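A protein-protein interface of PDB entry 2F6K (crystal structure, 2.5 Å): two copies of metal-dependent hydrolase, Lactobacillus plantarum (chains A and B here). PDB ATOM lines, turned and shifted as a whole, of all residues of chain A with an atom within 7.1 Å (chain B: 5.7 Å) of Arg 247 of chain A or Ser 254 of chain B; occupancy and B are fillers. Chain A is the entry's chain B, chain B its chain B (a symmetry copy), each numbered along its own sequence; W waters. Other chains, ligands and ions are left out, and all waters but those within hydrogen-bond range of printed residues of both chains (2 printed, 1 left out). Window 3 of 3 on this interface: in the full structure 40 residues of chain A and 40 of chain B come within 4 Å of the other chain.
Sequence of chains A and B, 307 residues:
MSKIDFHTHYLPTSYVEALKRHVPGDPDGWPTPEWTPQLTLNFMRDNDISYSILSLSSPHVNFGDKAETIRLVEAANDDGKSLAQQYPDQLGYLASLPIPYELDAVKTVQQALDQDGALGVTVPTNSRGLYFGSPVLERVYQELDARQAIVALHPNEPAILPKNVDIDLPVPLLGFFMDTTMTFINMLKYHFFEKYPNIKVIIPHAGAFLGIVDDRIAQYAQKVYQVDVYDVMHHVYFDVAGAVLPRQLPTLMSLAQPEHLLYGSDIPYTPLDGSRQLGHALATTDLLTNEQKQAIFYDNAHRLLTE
Printed residues of chain B within 4 Å of Ala 243 of chain A: Asp 215 (3.5 Å). Leu 245 of chain A touches none of the printed residues of chain B. Of chain B, only Gly 211 (3.6 Å), Asp 215 (2.8 Å), Tyr 230 (3.6 Å), Thr 251 (3.6 Å), Ser 254 (2.8 Å) and Leu 255 (3.4 Å) come within 4 Å of Arg 247 of chain A. Of the printed residues of chain B, Thr 251 of chain A touches Thr 251 (3.1 Å). Printed residues of chain A within 4 Å of Asp 215 of chain B: Ala 243, Pro 246 and Arg 247. Of the printed residues of chain A, Thr 251 of chain B touches Arg 247 and Thr 251. Of chain A, only Arg 247 (2.8 Å) comes within 4 Å of Ser 254 of chain B. Of the printed residues of chain A, Leu 255 of chain B touches Arg 247. The nearest printed residue of chain B that does not touch Arg 247 of chain A is Leu 252 of chain B (5.9 Å).
The backbone carbonyl oxygen (O) of Arg 247 of chain A lies within hydrogen-bond range of the side-chain hydroxyl (OG1) of Thr 251 of chain A (3.0 Å). The side-chain carboxylate of Asp 215 of chain B sits at hydrogen-bond distance from the side-chain hydroxyl of Tyr 230 of chain B (2.5 Å). O of Leu 255 of chain B sits close to NE2 of His 234 of chain B (3.4 Å). OG of Ser 254 of chain B is in hydrogen-bond range of O of Thr 251 of chain B.
Water W2 bridges the side-chain hydroxyl (OG1) of Thr 251 of chain A (2.7 Å) and the side-chain hydroxyl (OG1) of Thr 251 of chain B (2.8 Å). Water W1 lies within hydrogen-bond range of the side-chain hydroxyl of Thr 251 of chain B (2.7 Å), the side-chain hydroxyl of Thr 251 of chain A (2.8 Å) and the backbone carbonyl oxygen of Arg 247 of chain A (2.9 Å).
The guanidinium group of Arg 247 of chain A is in salt-bridge range of the side-chain carboxylate of Asp 215 of chain B. The guanidinium group of Arg 247 of chain A sits at hydrogen-bond distance from the side-chain hydroxyl of Ser 254 of chain B (2.8 Å). The side-chain hydroxyl of Thr 251 of chain A sits at hydrogen-bond distance from the side-chain hydroxyl of Thr 251 of chain B (3.1 Å).
Among the printed residues, merely in contact across the chains: Ala 243 of chain A with Asp 215 of chain B (3.5 Å), Pro 246 of chain A with Asp 215 of chain B (3.8 Å), Arg 247 of chain A with Gly 211 of chain B (3.6 Å), Arg 247 of chain A with Tyr 230 of chain B (3.6 Å), Arg 247 of chain A with Thr 251 of chain B (3.6 Å) and Arg 247 of chain A with Leu 255 of chain B (3.4 Å).
Thr 251 of chain B touches its own counterpart, Thr 251 of chain A. Of the 9 pairs that touch across the chains among the printed residues, 1 has its exchanged pair printed and touching as well.
Of the 11 printed residues of chain A, 4 touch a printed residue of chain B. Printed residues of chain A that touch a printed residue of chain B: Ala 243, Pro 246, Arg 247 and Thr 251. Hydrophobic or aromatic side chains of chain A that line the printed part of chain B: Ala 243 and Pro 246. Of the 12 printed residues of chain B, 6 touch a printed residue of chain A. Hydrophobic or aromatic side chains of chain B that line the printed part of chain A: Tyr 230 and Leu 255. Among the printed residues, Asp or Glu carboxylates within 4 Å of a Lys or Arg side-chain nitrogen of the other chain: Arg 247 of chain A with Asp 215 of chain B.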
ATOM      1  N   ALA A 243       7.836   4.326  -2.171  1.00  0.00           N
ATOM      2  CA  ALA A 243       8.820   4.308  -1.101  1.00  0.00           C
ATOM      3  C   ALA A 243       8.853   2.905  -0.497  1.00  0.00           C
ATOM      4  O   ALA A 243       8.464   2.702   0.650  1.00  0.00           O
ATOM      5  CB  ALA A 243       8.437   5.345  -0.051  1.00  0.00           C
ATOM      6  N   VAL A 244       9.327   1.942  -1.282  1.00  0.00           N
ATOM      7  CA  VAL A 244       9.381   0.551  -0.856  1.00  0.00           C
ATOM      8  C   VAL A 244      10.500   0.247   0.127  1.00  0.00           C
ATOM      9  O   VAL A 244      10.507  -0.808   0.757  1.00  0.00           O
ATOM     10  CB  VAL A 244       9.533  -0.391  -2.071  1.00  0.00           C
ATOM     11  CG1 VAL A 244       8.373  -0.175  -3.043  1.00  0.00           C
ATOM     12  CG2 VAL A 244      10.877  -0.146  -2.761  1.00  0.00           C
ATOM     13  N   LEU A 245      11.452   1.161   0.254  1.00  0.00           N
ATOM     14  CA  LEU A 245      12.564   0.961   1.170  1.00  0.00           C
ATOM     15  C   LEU A 245      12.445   1.982   2.282  1.00  0.00           C
ATOM     16  O   LEU A 245      11.950   3.080   2.055  1.00  0.00           O
ATOM     17  CB  LEU A 245      13.894   1.142   0.437  1.00  0.00           C
ATOM     18  CG  LEU A 245      14.197   0.103  -0.654  1.00  0.00           C
ATOM     19  CD1 LEU A 245      15.431   0.539  -1.449  1.00  0.00           C
ATOM     20  CD2 LEU A 245      14.407  -1.279  -0.022  1.00  0.00           C
ATOM     21  N   PRO A 246      12.914   1.646   3.496  1.00  0.00           N
ATOM     22  CA  PRO A 246      13.548   0.372   3.852  1.00  0.00           C
ATOM     23  C   PRO A 246      12.643  -0.661   4.530  1.00  0.00           C
ATOM     24  O   PRO A 246      13.123  -1.710   4.983  1.00  0.00           O
ATOM     25  CB  PRO A 246      14.664   0.815   4.782  1.00  0.00           C
ATOM     26  CG  PRO A 246      13.965   1.887   5.576  1.00  0.00           C
ATOM     27  CD  PRO A 246      13.207   2.670   4.517  1.00  0.00           C
ATOM     28  N   ARG A 247      11.345  -0.383   4.592  1.00  0.00           N
ATOM     29  CA  ARG A 247      10.435  -1.302   5.266  1.00  0.00           C
ATOM     30  C   ARG A 247       9.462  -2.131   4.435  1.00  0.00           C
ATOM     31  O   ARG A 247       9.333  -3.341   4.663  1.00  0.00           O
ATOM     32  CB  ARG A 247       9.645  -0.539   6.329  1.00  0.00           C
ATOM     33  CG  ARG A 247      10.478  -0.090   7.521  1.00  0.00           C
ATOM     34  CD  ARG A 247       9.784   1.038   8.272  1.00  0.00           C
ATOM     35  NE  ARG A 247      10.236   2.356   7.836  1.00  0.00           N
ATOM     36  CZ  ARG A 247      11.370   2.929   8.234  1.00  0.00           C
ATOM     37  NH1 ARG A 247      12.176   2.304   9.086  1.00  0.00           N
ATOM     38  NH2 ARG A 247      11.703   4.131   7.773  1.00  0.00           N
ATOM     39  N   GLN A 248       8.779  -1.495   3.484  1.00  0.00           N
ATOM     40  CA  GLN A 248       7.774  -2.181   2.673  1.00  0.00           C
ATOM     41  C   GLN A 248       8.232  -3.403   1.867  1.00  0.00           C
ATOM     42  O   GLN A 248       7.666  -4.493   2.015  1.00  0.00           O
ATOM     43  CB  GLN A 248       7.086  -1.189   1.732  1.00  0.00           C
ATOM     44  CG  GLN A 248       5.711  -1.664   1.286  1.00  0.00           C
ATOM     45  CD  GLN A 248       5.143  -0.848   0.145  1.00  0.00           C
ATOM     46  OE1 GLN A 248       3.949  -0.925  -0.147  1.00  0.00           O
ATOM     47  NE2 GLN A 248       5.996  -0.071  -0.515  1.00  0.00           N
ATOM     48  N   LEU A 249       9.240  -3.241   1.016  1.00  0.00           N
ATOM     49  CA  LEU A 249       9.710  -4.364   0.209  1.00  0.00           C
ATOM     50  C   LEU A 249      10.230  -5.527   1.061  1.00  0.00           C
ATOM     51  O   LEU A 249       9.870  -6.686   0.835  1.00  0.00           O
ATOM     52  CB  LEU A 249      10.782  -3.896  -0.778  1.00  0.00           C
ATOM     53  CG  LEU A 249      11.328  -4.947  -1.749  1.00  0.00           C
ATOM     54  CD1 LEU A 249      10.201  -5.810  -2.288  1.00  0.00           C
ATOM     55  CD2 LEU A 249      12.061  -4.244  -2.888  1.00  0.00           C
ATOM     56  N   PRO A 250      11.076  -5.237   2.058  1.00  0.00           N
ATOM     57  CA  PRO A 250      11.590  -6.322   2.899  1.00  0.00           C
ATOM     58  C   PRO A 250      10.469  -7.168   3.510  1.00  0.00           C
ATOM     59  O   PRO A 250      10.569  -8.389   3.573  1.00  0.00           O
ATOM     60  CB  PRO A 250      12.407  -5.578   3.956  1.00  0.00           C
ATOM     61  CG  PRO A 250      12.956  -4.428   3.176  1.00  0.00           C
ATOM     62  CD  PRO A 250      11.742  -3.962   2.381  1.00  0.00           C
ATOM     63  N   THR A 251       9.403  -6.523   3.961  1.00  0.00           N
ATOM     64  CA  THR A 251       8.289  -7.255   4.547  1.00  0.00           C
ATOM     65  C   THR A 251       7.579  -8.090   3.491  1.00  0.00           C
ATOM     66  O   THR A 251       7.157  -9.219   3.756  1.00  0.00           O
ATOM     67  CB  THR A 251       7.257  -6.308   5.159  1.00  0.00           C
ATOM     68  OG1 THR A 251       7.890  -5.485   6.148  1.00  0.00           O
ATOM     69  CG2 THR A 251       6.137  -7.103   5.797  1.00  0.00           C
ATOM     70  N   LEU A 252       7.443  -7.522   2.295  1.00  0.00           N
ATOM     71  CA  LEU A 252       6.774  -8.208   1.200  1.00  0.00           C
ATOM     72  C   LEU A 252       7.542  -9.449   0.755  1.00  0.00           C
ATOM     73  O   LEU A 252       6.950 -10.459   0.369  1.00  0.00           O
ATOM     74  CB  LEU A 252       6.593  -7.265   0.001  1.00  0.00           C
ATOM     75  CG  LEU A 252       6.049  -7.934  -1.268  1.00  0.00           C
ATOM     76  CD1 LEU A 252       4.603  -8.348  -1.027  1.00  0.00           C
ATOM     77  CD2 LEU A 252       6.146  -6.989  -2.459  1.00  0.00           C
ATOM     78  N   LEU A 287      19.704  -3.937   1.624  1.00  0.00           N
ATOM     79  CA  LEU A 287      18.585  -4.819   1.934  1.00  0.00           C
ATOM     80  C   LEU A 287      18.310  -5.831   0.820  1.00  0.00           C
ATOM     81  O   LEU A 287      17.464  -6.718   0.963  1.00  0.00           O
ATOM     82  CB  LEU A 287      17.340  -3.971   2.190  1.00  0.00           C
ATOM     83  CG  LEU A 287      17.560  -2.958   3.312  1.00  0.00           C
ATOM     84  CD1 LEU A 287      16.418  -1.964   3.354  1.00  0.00           C
ATOM     85  CD2 LEU A 287      17.696  -3.701   4.635  1.00  0.00           C
ATOM     86  N   GLY B 211       3.673   1.603   9.790  1.00  0.00           N
ATOM     87  CA  GLY B 211       4.933   1.011   9.387  1.00  0.00           C
ATOM     88  C   GLY B 211       5.152   0.994   7.888  1.00  0.00           C
ATOM     89  O   GLY B 211       6.266   0.759   7.429  1.00  0.00           O
ATOM     90  N   ASP B 215       6.877   6.175   5.444  1.00  0.00           N
ATOM     91  CA  ASP B 215       7.863   6.374   4.391  1.00  0.00           C
ATOM     92  C   ASP B 215       7.261   7.011   3.149  1.00  0.00           C
ATOM     93  O   ASP B 215       7.934   7.747   2.434  1.00  0.00           O
ATOM     94  CB  ASP B 215       8.509   5.036   4.044  1.00  0.00           C
ATOM     95  CG  ASP B 215       9.402   4.517   5.164  1.00  0.00           C
ATOM     96  OD1 ASP B 215       9.537   3.280   5.290  1.00  0.00           O
ATOM     97  OD2 ASP B 215       9.975   5.346   5.908  1.00  0.00           O
ATOM     98  N   TYR B 230       9.057  10.710  11.417  1.00  0.00           N
ATOM     99  CA  TYR B 230       9.993   9.837  12.128  1.00  0.00           C
ATOM    100  C   TYR B 230      10.215  10.283  13.578  1.00  0.00           C
ATOM    101  O   TYR B 230      10.326   9.445  14.477  1.00  0.00           O
ATOM    102  CB  TYR B 230      11.323   9.774  11.378  1.00  0.00           C
ATOM    103  CG  TYR B 230      11.159   9.226   9.979  1.00  0.00           C
ATOM    104  CD1 TYR B 230      10.764   7.902   9.774  1.00  0.00           C
ATOM    105  CD2 TYR B 230      11.328  10.047   8.857  1.00  0.00           C
ATOM    106  CE1 TYR B 230      10.536   7.407   8.491  1.00  0.00           C
ATOM    107  CE2 TYR B 230      11.106   9.564   7.568  1.00  0.00           C
ATOM    108  CZ  TYR B 230      10.708   8.241   7.391  1.00  0.00           C
ATOM    109  OH  TYR B 230      10.486   7.743   6.122  1.00  0.00           O
ATOM    110  N   HIS B 234       8.925   8.246  17.291  1.00  0.00           N
ATOM    111  CA  HIS B 234       9.782   8.032  18.453  1.00  0.00           C
ATOM    112  C   HIS B 234       9.090   8.574  19.704  1.00  0.00           C
ATOM    113  O   HIS B 234       9.270   8.060  20.812  1.00  0.00           O
ATOM    114  CB  HIS B 234      11.104   8.772  18.273  1.00  0.00           C
ATOM    115  CG  HIS B 234      12.079   8.064  17.388  1.00  0.00           C
ATOM    116  ND1 HIS B 234      13.083   8.722  16.713  1.00  0.00           N
ATOM    117  CD2 HIS B 234      12.219   6.751  17.085  1.00  0.00           C
ATOM    118  CE1 HIS B 234      13.799   7.848  16.031  1.00  0.00           C
ATOM    119  NE2 HIS B 234      13.296   6.644  16.240  1.00  0.00           N
ATOM    120  N   LEU B 249       5.320  -6.123  13.970  1.00  0.00           N
ATOM    121  CA  LEU B 249       6.165  -5.602  15.041  1.00  0.00           C
ATOM    122  C   LEU B 249       7.603  -5.335  14.582  1.00  0.00           C
ATOM    123  O   LEU B 249       8.163  -4.268  14.849  1.00  0.00           O
ATOM    124  CB  LEU B 249       6.149  -6.553  16.240  1.00  0.00           C
ATOM    125  CG  LEU B 249       6.934  -6.112  17.478  1.00  0.00           C
ATOM    126  CD1 LEU B 249       6.717  -4.634  17.747  1.00  0.00           C
ATOM    127  CD2 LEU B 249       6.494  -6.949  18.676  1.00  0.00           C
ATOM    128  N   PRO B 250       8.218  -6.294  13.878  1.00  0.00           N
ATOM    129  CA  PRO B 250       9.593  -6.074  13.416  1.00  0.00           C
ATOM    130  C   PRO B 250       9.736  -4.780  12.609  1.00  0.00           C
ATOM    131  O   PRO B 250      10.710  -4.051  12.762  1.00  0.00           O
ATOM    132  CB  PRO B 250       9.877  -7.322  12.581  1.00  0.00           C
ATOM    133  CG  PRO B 250       9.114  -8.374  13.317  1.00  0.00           C
ATOM    134  CD  PRO B 250       7.788  -7.677  13.603  1.00  0.00           C
ATOM    135  N   THR B 251       8.768  -4.494  11.750  1.00  0.00           N
ATOM    136  CA  THR B 251       8.824  -3.278  10.951  1.00  0.00           C
ATOM    137  C   THR B 251       8.671  -2.047  11.834  1.00  0.00           C
ATOM    138  O   THR B 251       9.330  -1.027  11.617  1.00  0.00           O
ATOM    139  CB  THR B 251       7.708  -3.241   9.908  1.00  0.00           C
ATOM    140  OG1 THR B 251       7.803  -4.397   9.065  1.00  0.00           O
ATOM    141  CG2 THR B 251       7.823  -1.986   9.068  1.00  0.00           C
ATOM    142  N   LEU B 252       7.789  -2.149  12.826  1.00  0.00           N
ATOM    143  CA  LEU B 252       7.538  -1.042  13.737  1.00  0.00           C
ATOM    144  C   LEU B 252       8.765  -0.715  14.582  1.00  0.00           C
ATOM    145  O   LEU B 252       9.026   0.447  14.901  1.00  0.00           O
ATOM    146  CB  LEU B 252       6.354  -1.360  14.661  1.00  0.00           C
ATOM    147  CG  LEU B 252       6.109  -0.330  15.772  1.00  0.00           C
ATOM    148  CD1 LEU B 252       5.623   0.969  15.143  1.00  0.00           C
ATOM    149  CD2 LEU B 252       5.093  -0.854  16.778  1.00  0.00           C
ATOM    150  N   MET B 253       9.532  -1.732  14.937  1.00  0.00           N
ATOM    151  CA  MET B 253      10.700  -1.489  15.768  1.00  0.00           C
ATOM    152  C   MET B 253      11.811  -0.674  15.115  1.00  0.00           C
ATOM    153  O   MET B 253      12.699  -0.181  15.804  1.00  0.00           O
ATOM    154  CB  MET B 253      11.232  -2.808  16.318  1.00  0.00           C
ATOM    155  CG  MET B 253      10.190  -3.513  17.164  1.00  0.00           C
ATOM    156  SD  MET B 253      10.780  -5.141  17.996  1.00  0.00           S
ATOM    157  CE  MET B 253      11.188  -6.178  16.439  1.00  0.00           C
ATOM    158  N   SER B 254      11.773  -0.518  13.795  1.00  0.00           N
ATOM    159  CA  SER B 254      12.788   0.298  13.137  1.00  0.00           C
ATOM    160  C   SER B 254      12.302   1.755  13.137  1.00  0.00           C
ATOM    161  O   SER B 254      13.000   2.648  12.660  1.00  0.00           O
ATOM    162  CB  SER B 254      13.024  -0.172  11.697  1.00  0.00           C
ATOM    163  OG  SER B 254      11.905   0.113  10.875  1.00  0.00           O
ATOM    164  N   LEU B 255      11.107   1.989  13.681  1.00  0.00           N
ATOM    165  CA  LEU B 255      10.523   3.331  13.727  1.00  0.00           C
ATOM    166  C   LEU B 255      10.225   3.801  15.137  1.00  0.00           C
ATOM    167  O   LEU B 255      10.391   4.979  15.458  1.00  0.00           O
ATOM    168  CB  LEU B 255       9.225   3.377  12.920  1.00  0.00           C
ATOM    169  CG  LEU B 255       9.354   3.249  11.399  1.00  0.00           C
ATOM    170  CD1 LEU B 255       8.021   2.870  10.804  1.00  0.00           C
ATOM    171  CD2 LEU B 255       9.859   4.554  10.815  1.00  0.00           C
ATOM    172  N   ALA B 256       9.783   2.873  15.974  1.00  0.00           N
ATOM    173  CA  ALA B 256       9.438   3.188  17.349  1.00  0.00           C
ATOM    174  C   ALA B 256      10.626   3.122  18.294  1.00  0.00           C
ATOM    175  O   ALA B 256      11.641   2.489  18.005  1.00  0.00           O
ATOM    176  CB  ALA B 256       8.345   2.243  17.841  1.00  0.00           C
HETATM  177  O   HOH W   1       9.926  -3.947   7.403  1.00  0.00           O
HETATM  178  O   HOH W   2       8.300  -7.096   8.318  1.00  0.00           O
